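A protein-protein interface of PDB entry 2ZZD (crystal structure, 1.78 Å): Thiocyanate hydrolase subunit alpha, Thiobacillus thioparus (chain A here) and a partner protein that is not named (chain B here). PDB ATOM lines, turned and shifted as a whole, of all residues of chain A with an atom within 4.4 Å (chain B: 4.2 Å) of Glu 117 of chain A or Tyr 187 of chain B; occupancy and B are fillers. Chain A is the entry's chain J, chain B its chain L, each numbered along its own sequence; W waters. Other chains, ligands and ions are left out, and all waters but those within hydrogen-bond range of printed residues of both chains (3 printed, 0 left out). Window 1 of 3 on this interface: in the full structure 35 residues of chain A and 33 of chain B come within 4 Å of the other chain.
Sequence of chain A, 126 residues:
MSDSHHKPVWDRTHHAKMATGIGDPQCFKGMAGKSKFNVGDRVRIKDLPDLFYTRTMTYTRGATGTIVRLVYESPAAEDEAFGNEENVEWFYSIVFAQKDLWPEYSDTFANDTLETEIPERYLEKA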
ATOM      1  N   VAL A  71     -31.814  -2.293  -0.733  1.00  0.00           N
ATOM      2  CA  VAL A  71     -31.432  -0.943  -0.356  1.00  0.00           C
ATOM      3  C   VAL A  71     -32.347  -0.143   0.567  1.00  0.00           C
ATOM      4  O   VAL A  71     -31.857   0.546   1.464  1.00  0.00           O
ATOM      5  CB  VAL A  71     -31.113  -0.111  -1.620  1.00  0.00           C
ATOM      6  CG1 VAL A  71     -29.882  -0.695  -2.310  1.00  0.00           C
ATOM      7  CG2 VAL A  71     -32.295  -0.128  -2.584  1.00  0.00           C
ATOM      8  N   TYR A  72     -33.657  -0.223   0.355  1.00  0.00           N
ATOM      9  CA  TYR A  72     -34.618   0.512   1.185  1.00  0.00           C
ATOM     10  C   TYR A  72     -36.027   0.233   0.689  1.00  0.00           C
ATOM     11  O   TYR A  72     -36.218  -0.509  -0.272  1.00  0.00           O
ATOM     12  CB  TYR A  72     -34.342   2.021   1.116  1.00  0.00           C
ATOM     13  CG  TYR A  72     -34.201   2.543  -0.298  1.00  0.00           C
ATOM     14  CD1 TYR A  72     -35.315   2.680  -1.130  1.00  0.00           C
ATOM     15  CD2 TYR A  72     -32.941   2.827  -0.827  1.00  0.00           C
ATOM     16  CE1 TYR A  72     -35.173   3.081  -2.462  1.00  0.00           C
ATOM     17  CE2 TYR A  72     -32.787   3.220  -2.154  1.00  0.00           C
ATOM     18  CZ  TYR A  72     -33.905   3.342  -2.968  1.00  0.00           C
ATOM     19  OH  TYR A  72     -33.744   3.684  -4.293  1.00  0.00           O
ATOM     20  N   TYR A  92     -34.337  -3.064  -4.830  1.00  0.00           N
ATOM     21  CA  TYR A  92     -33.180  -3.950  -4.854  1.00  0.00           C
ATOM     22  C   TYR A  92     -32.058  -3.437  -5.749  1.00  0.00           C
ATOM     23  O   TYR A  92     -32.317  -2.890  -6.819  1.00  0.00           O
ATOM     24  CB  TYR A  92     -33.606  -5.321  -5.381  1.00  0.00           C
ATOM     25  CG  TYR A  92     -34.722  -5.984  -4.604  1.00  0.00           C
ATOM     26  CD1 TYR A  92     -34.438  -6.944  -3.634  1.00  0.00           C
ATOM     27  CD2 TYR A  92     -36.061  -5.670  -4.853  1.00  0.00           C
ATOM     28  CE1 TYR A  92     -35.455  -7.583  -2.932  1.00  0.00           C
ATOM     29  CE2 TYR A  92     -37.090  -6.303  -4.154  1.00  0.00           C
ATOM     30  CZ  TYR A  92     -36.776  -7.261  -3.196  1.00  0.00           C
ATOM     31  OH  TYR A  92     -37.773  -7.912  -2.508  1.00  0.00           O
ATOM     32  N   SER A  93     -30.810  -3.608  -5.315  1.00  0.00           N
ATOM     33  CA  SER A  93     -29.689  -3.210  -6.156  1.00  0.00           C
ATOM     34  C   SER A  93     -29.349  -4.501  -6.888  1.00  0.00           C
ATOM     35  O   SER A  93     -29.122  -5.541  -6.264  1.00  0.00           O
ATOM     36  CB  SER A  93     -28.499  -2.731  -5.332  1.00  0.00           C
ATOM     37  OG  SER A  93     -27.591  -2.024  -6.170  1.00  0.00           O
ATOM     38  N   THR A 116     -27.623  -1.358 -10.817  1.00  0.00           N
ATOM     39  CA  THR A 116     -28.654  -0.330 -10.774  1.00  0.00           C
ATOM     40  C   THR A 116     -29.800  -0.807  -9.878  1.00  0.00           C
ATOM     41  O   THR A 116     -29.857  -1.984  -9.521  1.00  0.00           O
ATOM     42  CB  THR A 116     -29.146   0.017 -12.203  1.00  0.00           C
ATOM     43  OG1 THR A 116     -29.924   1.221 -12.165  1.00  0.00           O
ATOM     44  CG2 THR A 116     -29.981  -1.112 -12.787  1.00  0.00           C
ATOM     45  N   GLU A 117     -30.699   0.100  -9.503  1.00  0.00           N
ATOM     46  CA  GLU A 117     -31.800  -0.248  -8.608  1.00  0.00           C
ATOM     47  C   GLU A 117     -33.160  -0.406  -9.274  1.00  0.00           C
ATOM     48  O   GLU A 117     -33.553   0.385 -10.134  1.00  0.00           O
ATOM     49  CB  GLU A 117     -31.886   0.774  -7.472  1.00  0.00           C
ATOM     50  CG  GLU A 117     -30.699   0.673  -6.515  1.00  0.00           C
ATOM     51  CD  GLU A 117     -30.697   1.728  -5.428  1.00  0.00           C
ATOM     52  OE1 GLU A 117     -31.614   2.580  -5.401  1.00  0.00           O
ATOM     53  OE2 GLU A 117     -29.770   1.695  -4.588  1.00  0.00           O
ATOM     54  N   ILE A 118     -33.885  -1.433  -8.848  1.00  0.00           N
ATOM     55  CA  ILE A 118     -35.192  -1.731  -9.420  1.00  0.00           C
ATOM     56  C   ILE A 118     -36.184  -2.146  -8.334  1.00  0.00           C
ATOM     57  O   ILE A 118     -35.860  -2.955  -7.464  1.00  0.00           O
ATOM     58  CB  ILE A 118     -35.054  -2.860 -10.470  1.00  0.00           C
ATOM     59  CG1 ILE A 118     -34.097  -2.406 -11.579  1.00  0.00           C
ATOM     60  CG2 ILE A 118     -36.417  -3.223 -11.045  1.00  0.00           C
ATOM     61  CD1 ILE A 118     -33.705  -3.483 -12.560  1.00  0.00           C
ATOM     62  N   ARG B 114     -24.431   5.602  -0.956  1.00  0.00           N
ATOM     63  CA  ARG B 114     -23.745   4.326  -0.935  1.00  0.00           C
ATOM     64  C   ARG B 114     -22.334   4.622  -1.424  1.00  0.00           C
ATOM     65  O   ARG B 114     -22.144   5.402  -2.360  1.00  0.00           O
ATOM     66  CB  ARG B 114     -24.429   3.294  -1.837  1.00  0.00           C
ATOM     67  CG  ARG B 114     -25.612   2.565  -1.181  1.00  0.00           C
ATOM     68  CD  ARG B 114     -25.910   1.245  -1.898  1.00  0.00           C
ATOM     69  NE  ARG B 114     -24.772   0.333  -1.818  1.00  0.00           N
ATOM     70  CZ  ARG B 114     -24.434  -0.539  -2.765  1.00  0.00           C
ATOM     71  NH1 ARG B 114     -25.153  -0.628  -3.878  1.00  0.00           N
ATOM     72  NH2 ARG B 114     -23.363  -1.309  -2.608  1.00  0.00           N
ATOM     73  N   LEU B 116     -19.015   3.110  -3.062  1.00  0.00           N
ATOM     74  CA  LEU B 116     -18.549   1.976  -3.860  1.00  0.00           C
ATOM     75  C   LEU B 116     -17.038   1.824  -3.739  1.00  0.00           C
ATOM     76  O   LEU B 116     -16.286   2.677  -4.201  1.00  0.00           O
ATOM     77  CB  LEU B 116     -18.940   2.193  -5.321  1.00  0.00           C
ATOM     78  CG  LEU B 116     -20.442   2.372  -5.557  1.00  0.00           C
ATOM     79  CD1 LEU B 116     -20.701   2.730  -7.018  1.00  0.00           C
ATOM     80  CD2 LEU B 116     -21.174   1.094  -5.178  1.00  0.00           C
ATOM     81  N   VAL B 126     -19.676   6.111 -12.120  1.00  0.00           N
ATOM     82  CA  VAL B 126     -21.085   6.448 -11.945  1.00  0.00           C
ATOM     83  C   VAL B 126     -21.717   7.357 -13.000  1.00  0.00           C
ATOM     84  O   VAL B 126     -21.054   8.208 -13.591  1.00  0.00           O
ATOM     85  CB  VAL B 126     -21.263   7.111 -10.556  1.00  0.00           C
ATOM     86  CG1 VAL B 126     -22.729   7.281 -10.223  1.00  0.00           C
ATOM     87  CG2 VAL B 126     -20.561   6.269  -9.493  1.00  0.00           C
ATOM     88  N   PRO B 135     -24.530  12.830  -5.900  1.00  0.00           N
ATOM     89  CA  PRO B 135     -24.505  12.995  -4.440  1.00  0.00           C
ATOM     90  C   PRO B 135     -24.146  14.416  -4.004  1.00  0.00           C
ATOM     91  O   PRO B 135     -23.159  14.628  -3.302  1.00  0.00           O
ATOM     92  CB  PRO B 135     -23.461  11.973  -4.007  1.00  0.00           C
ATOM     93  CG  PRO B 135     -22.450  12.067  -5.127  1.00  0.00           C
ATOM     94  CD  PRO B 135     -23.359  12.057  -6.356  1.00  0.00           C
ATOM     95  N   ALA B 179     -22.284   2.099 -12.285  1.00  0.00           N
ATOM     96  CA  ALA B 179     -23.421   2.205 -11.383  1.00  0.00           C
ATOM     97  C   ALA B 179     -24.341   3.272 -11.953  1.00  0.00           C
ATOM     98  O   ALA B 179     -23.925   4.420 -12.145  1.00  0.00           O
ATOM     99  CB  ALA B 179     -22.958   2.596  -9.982  1.00  0.00           C
ATOM    100  N   SER B 181     -27.353   5.531 -11.254  1.00  0.00           N
ATOM    101  CA  SER B 181     -28.112   6.132 -10.140  1.00  0.00           C
ATOM    102  C   SER B 181     -29.552   6.482 -10.514  1.00  0.00           C
ATOM    103  O   SER B 181     -29.926   7.650 -10.498  1.00  0.00           O
ATOM    104  CB  SER B 181     -27.401   7.408  -9.673  1.00  0.00           C
ATOM    105  OG  SER B 181     -25.993   7.243  -9.660  1.00  0.00           O
ATOM    106  N   ASN B 182     -30.368   5.472 -10.790  1.00  0.00           N
ATOM    107  CA  ASN B 182     -31.738   5.703 -11.233  1.00  0.00           C
ATOM    108  C   ASN B 182     -32.846   5.849 -10.186  1.00  0.00           C
ATOM    109  O   ASN B 182     -33.929   6.319 -10.518  1.00  0.00           O
ATOM    110  CB  ASN B 182     -32.128   4.596 -12.208  1.00  0.00           C
ATOM    111  CG  ASN B 182     -32.223   3.245 -11.528  1.00  0.00           C
ATOM    112  OD1 ASN B 182     -31.472   2.959 -10.593  1.00  0.00           O
ATOM    113  ND2 ASN B 182     -33.134   2.401 -12.004  1.00  0.00           N
ATOM    114  N   GLN B 183     -32.614   5.442  -8.943  1.00  0.00           N
ATOM    115  CA  GLN B 183     -33.676   5.582  -7.952  1.00  0.00           C
ATOM    116  C   GLN B 183     -33.237   6.563  -6.863  1.00  0.00           C
ATOM    117  O   GLN B 183     -32.719   7.631  -7.182  1.00  0.00           O
ATOM    118  CB  GLN B 183     -34.057   4.216  -7.366  1.00  0.00           C
ATOM    119  CG  GLN B 183     -34.426   3.138  -8.419  1.00  0.00           C
ATOM    120  CD  GLN B 183     -35.738   3.398  -9.175  1.00  0.00           C
ATOM    121  OE1 GLN B 183     -36.513   4.292  -8.832  1.00  0.00           O
ATOM    122  NE2 GLN B 183     -35.993   2.588 -10.201  1.00  0.00           N
ATOM    123  N   LYS B 184     -33.410   6.221  -5.592  1.00  0.00           N
ATOM    124  CA  LYS B 184     -33.043   7.166  -4.535  1.00  0.00           C
ATOM    125  C   LYS B 184     -31.631   7.078  -3.962  1.00  0.00           C
ATOM    126  O   LYS B 184     -31.266   7.857  -3.080  1.00  0.00           O
ATOM    127  CB  LYS B 184     -34.075   7.098  -3.408  1.00  0.00           C
ATOM    128  CG  LYS B 184     -35.439   7.617  -3.849  1.00  0.00           C
ATOM    129  CD  LYS B 184     -36.466   7.573  -2.729  1.00  0.00           C
ATOM    130  CE  LYS B 184     -37.794   8.146  -3.206  1.00  0.00           C
ATOM    131  NZ  LYS B 184     -38.840   8.117  -2.140  1.00  0.00           N
ATOM    132  N   THR B 185     -30.833   6.142  -4.462  1.00  0.00           N
ATOM    133  CA  THR B 185     -29.458   6.006  -3.998  1.00  0.00           C
ATOM    134  C   THR B 185     -28.518   6.896  -4.815  1.00  0.00           C
ATOM    135  O   THR B 185     -28.674   7.038  -6.028  1.00  0.00           O
ATOM    136  CB  THR B 185     -28.967   4.541  -4.115  1.00  0.00           C
ATOM    137  OG1 THR B 185     -29.596   3.747  -3.104  1.00  0.00           O
ATOM    138  CG2 THR B 185     -27.446   4.457  -3.950  1.00  0.00           C
ATOM    139  N   ARG B 186     -27.555   7.505  -4.131  1.00  0.00           N
ATOM    140  CA  ARG B 186     -26.541   8.336  -4.774  1.00  0.00           C
ATOM    141  C   ARG B 186     -25.232   7.654  -4.394  1.00  0.00           C
ATOM    142  O   ARG B 186     -25.124   7.092  -3.302  1.00  0.00           O
ATOM    143  CB  ARG B 186     -26.574   9.769  -4.241  1.00  0.00           C
ATOM    144  CG  ARG B 186     -27.875  10.499  -4.540  1.00  0.00           C
ATOM    145  CD  ARG B 186     -28.118  10.631  -6.046  1.00  0.00           C
ATOM    146  NE  ARG B 186     -29.404  11.269  -6.322  1.00  0.00           N
ATOM    147  CZ  ARG B 186     -30.541  10.611  -6.538  1.00  0.00           C
ATOM    148  NH1 ARG B 186     -30.569   9.284  -6.528  1.00  0.00           N
ATOM    149  NH2 ARG B 186     -31.668  11.286  -6.742  1.00  0.00           N
ATOM    150  N   TYR B 187     -24.243   7.696  -5.282  1.00  0.00           N
ATOM    151  CA  TYR B 187     -22.971   7.023  -5.032  1.00  0.00           C
ATOM    152  C   TYR B 187     -21.738   7.903  -5.112  1.00  0.00           C
ATOM    153  O   TYR B 187     -21.732   8.916  -5.808  1.00  0.00           O
ATOM    154  CB  TYR B 187     -22.728   5.940  -6.088  1.00  0.00           C
ATOM    155  CG  TYR B 187     -23.830   4.941  -6.319  1.00  0.00           C
ATOM    156  CD1 TYR B 187     -23.920   3.788  -5.545  1.00  0.00           C
ATOM    157  CD2 TYR B 187     -24.737   5.112  -7.366  1.00  0.00           C
ATOM    158  CE1 TYR B 187     -24.877   2.819  -5.810  1.00  0.00           C
ATOM    159  CE2 TYR B 187     -25.705   4.150  -7.641  1.00  0.00           C
ATOM    160  CZ  TYR B 187     -25.766   3.006  -6.860  1.00  0.00           C
ATOM    161  OH  TYR B 187     -26.706   2.043  -7.129  1.00  0.00           O
ATOM    162  N   ILE B 188     -20.700   7.501  -4.380  1.00  0.00           N
ATOM    163  CA  ILE B 188     -19.391   8.126  -4.516  1.00  0.00           C
ATOM    164  C   ILE B 188     -18.464   6.923  -4.602  1.00  0.00           C
ATOM    165  O   ILE B 188     -18.725   5.875  -4.001  1.00  0.00           O
ATOM    166  CB  ILE B 188     -18.934   9.062  -3.353  1.00  0.00           C
ATOM    167  CG1 ILE B 188     -18.972   8.354  -2.003  1.00  0.00           C
ATOM    168  CG2 ILE B 188     -19.739  10.347  -3.386  1.00  0.00           C
ATOM    169  CD1 ILE B 188     -18.292   9.192  -0.895  1.00  0.00           C
HETATM  170  O   HOH W   1     -27.445   0.508  -5.190  1.00  0.00           O
HETATM  171  O   HOH W   2     -30.398   5.092  -7.322  1.00  0.00           O
HETATM  172  O   HOH W   3     -29.040   2.958  -8.409  1.00  0.00           O
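The backbone NH (N) of Arg 114 of chain B sits at hydrogen-bond distance from the backbone carbonyl oxygen (O) of Arg 186 of chain B, 2.9 Å away.
The backbone carbonyl oxygen (O) of Gln 183 of chain B lies within hydrogen-bond range of the guanidinium group (NH1) of Arg 186 of chain B, at 2.8 Å.
The side-chain amide nitrogen (ND2) of Asn 182 of chain B sits close to the side-chain amide nitrogen (NE2) of Gln 183 of chain B.
The backbone carbonyl oxygen of Arg 114 of chain B sits at hydrogen-bond distance from the backbone NH of Ile 188 of chain B, 3.3 Å away.
The side-chain hydroxyl of Tyr 72 of chain A sits at hydrogen-bond distance from the side-chain carboxylate of Glu 117 of chain A (2.6 Å).
Of the printed residues of chain B, Ser 93 of chain A touches Arg 114.
Of the printed residues of chain B, Thr 116 of chain A touches Asn 182.
Printed residues of chain B within 4 Å of Glu 117 of chain A: Asn 182 (2.8 Å), Gln 183 (3.3 Å), Thr 185 (2.5 Å) and Tyr 187 (3.996 Å).
Leu 116 of chain B touches none of the printed residues of chain A.
Of the printed residues of chain A, Gln 183 of chain B touches Tyr 72 (3.1 Å) and Glu 117 (3.3 Å).
Printed residues of chain A within 4 Å of Lys 184 of chain B: Tyr 72.
Printed residues of chain A within 4 Å of Tyr 187 of chain B: Glu 117 (3.996 Å).
The nearest printed residue of chain A that does not touch Tyr 187 of chain B is Ser 93 of chain A (4.3 Å).
Printed residues of chain B that touch a printed residue of chain A: Arg 114, Asn 182, Gln 183, Lys 184, Thr 185 and Tyr 187.
Hydrophobic or aromatic side chains of chain B that line the printed part of chain A: Tyr 187.
Of the 7 printed residues of chain A, 4 touch a printed residue of chain B.
Among the printed residues, 9 pairs touch across the chains.
Among the printed residues, no Asp or Glu carboxylate lies within 4 Å of a Lys or Arg side-chain nitrogen of the other chain.
OH of Tyr 72 of chain A touches CB of Gln 183 of chain B, at 3.1 Å.
Tyr 72 of chain A touches Thr 185 of chain B.
Ser 93 of chain A touches Arg 114 of chain B (OG to NH1, 3.6 Å).
Glu 117 of chain A touches Tyr 187 of chain B (OE2 to OH, 3.996 Å).
Water W1 lies within hydrogen-bond range of OH of Tyr 187 of chain B (2.6 Å), OE2 of Glu 117 of chain A (2.7 Å), OG of Ser 93 of chain A (2.7 Å) and NH1 of Arg 114 of chain B (2.9 Å).
Water W2 lies within hydrogen-bond range of the backbone NH of Gln 183 of chain B, the backbone carbonyl oxygen of Thr 185 of chain B, the side-chain carboxylate of Glu 117 of chain A and the backbone NH of Asn 182 of chain B.
Water W3 lies within hydrogen-bond range of OH of Tyr 187 of chain B (2.8 Å), OD1 of Asn 182 of chain B (3.3 Å) and N of Glu 117 of chain A (3.5 Å).
The side-chain carboxylate of Glu 117 of chain A is in hydrogen-bond range of the side-chain hydroxyl of Thr 185 of chain B (2.5 Å).
NE2 of Gln 183 of chain B sits at hydrogen-bond distance from O of Glu 117 of chain A (3.3 Å).
OG1 of Thr 116 of chain A is in hydrogen-bond range of OD1 of Asn 182 of chain B (2.8 Å).
The backbone NH of Lys 184 of chain B sits at hydrogen-bond distance from the side-chain hydroxyl of Tyr 72 of chain A (2.9 Å).
ND2 of Asn 182 of chain B is in hydrogen-bond range of O of Glu 117 of chain A (2.8 Å).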
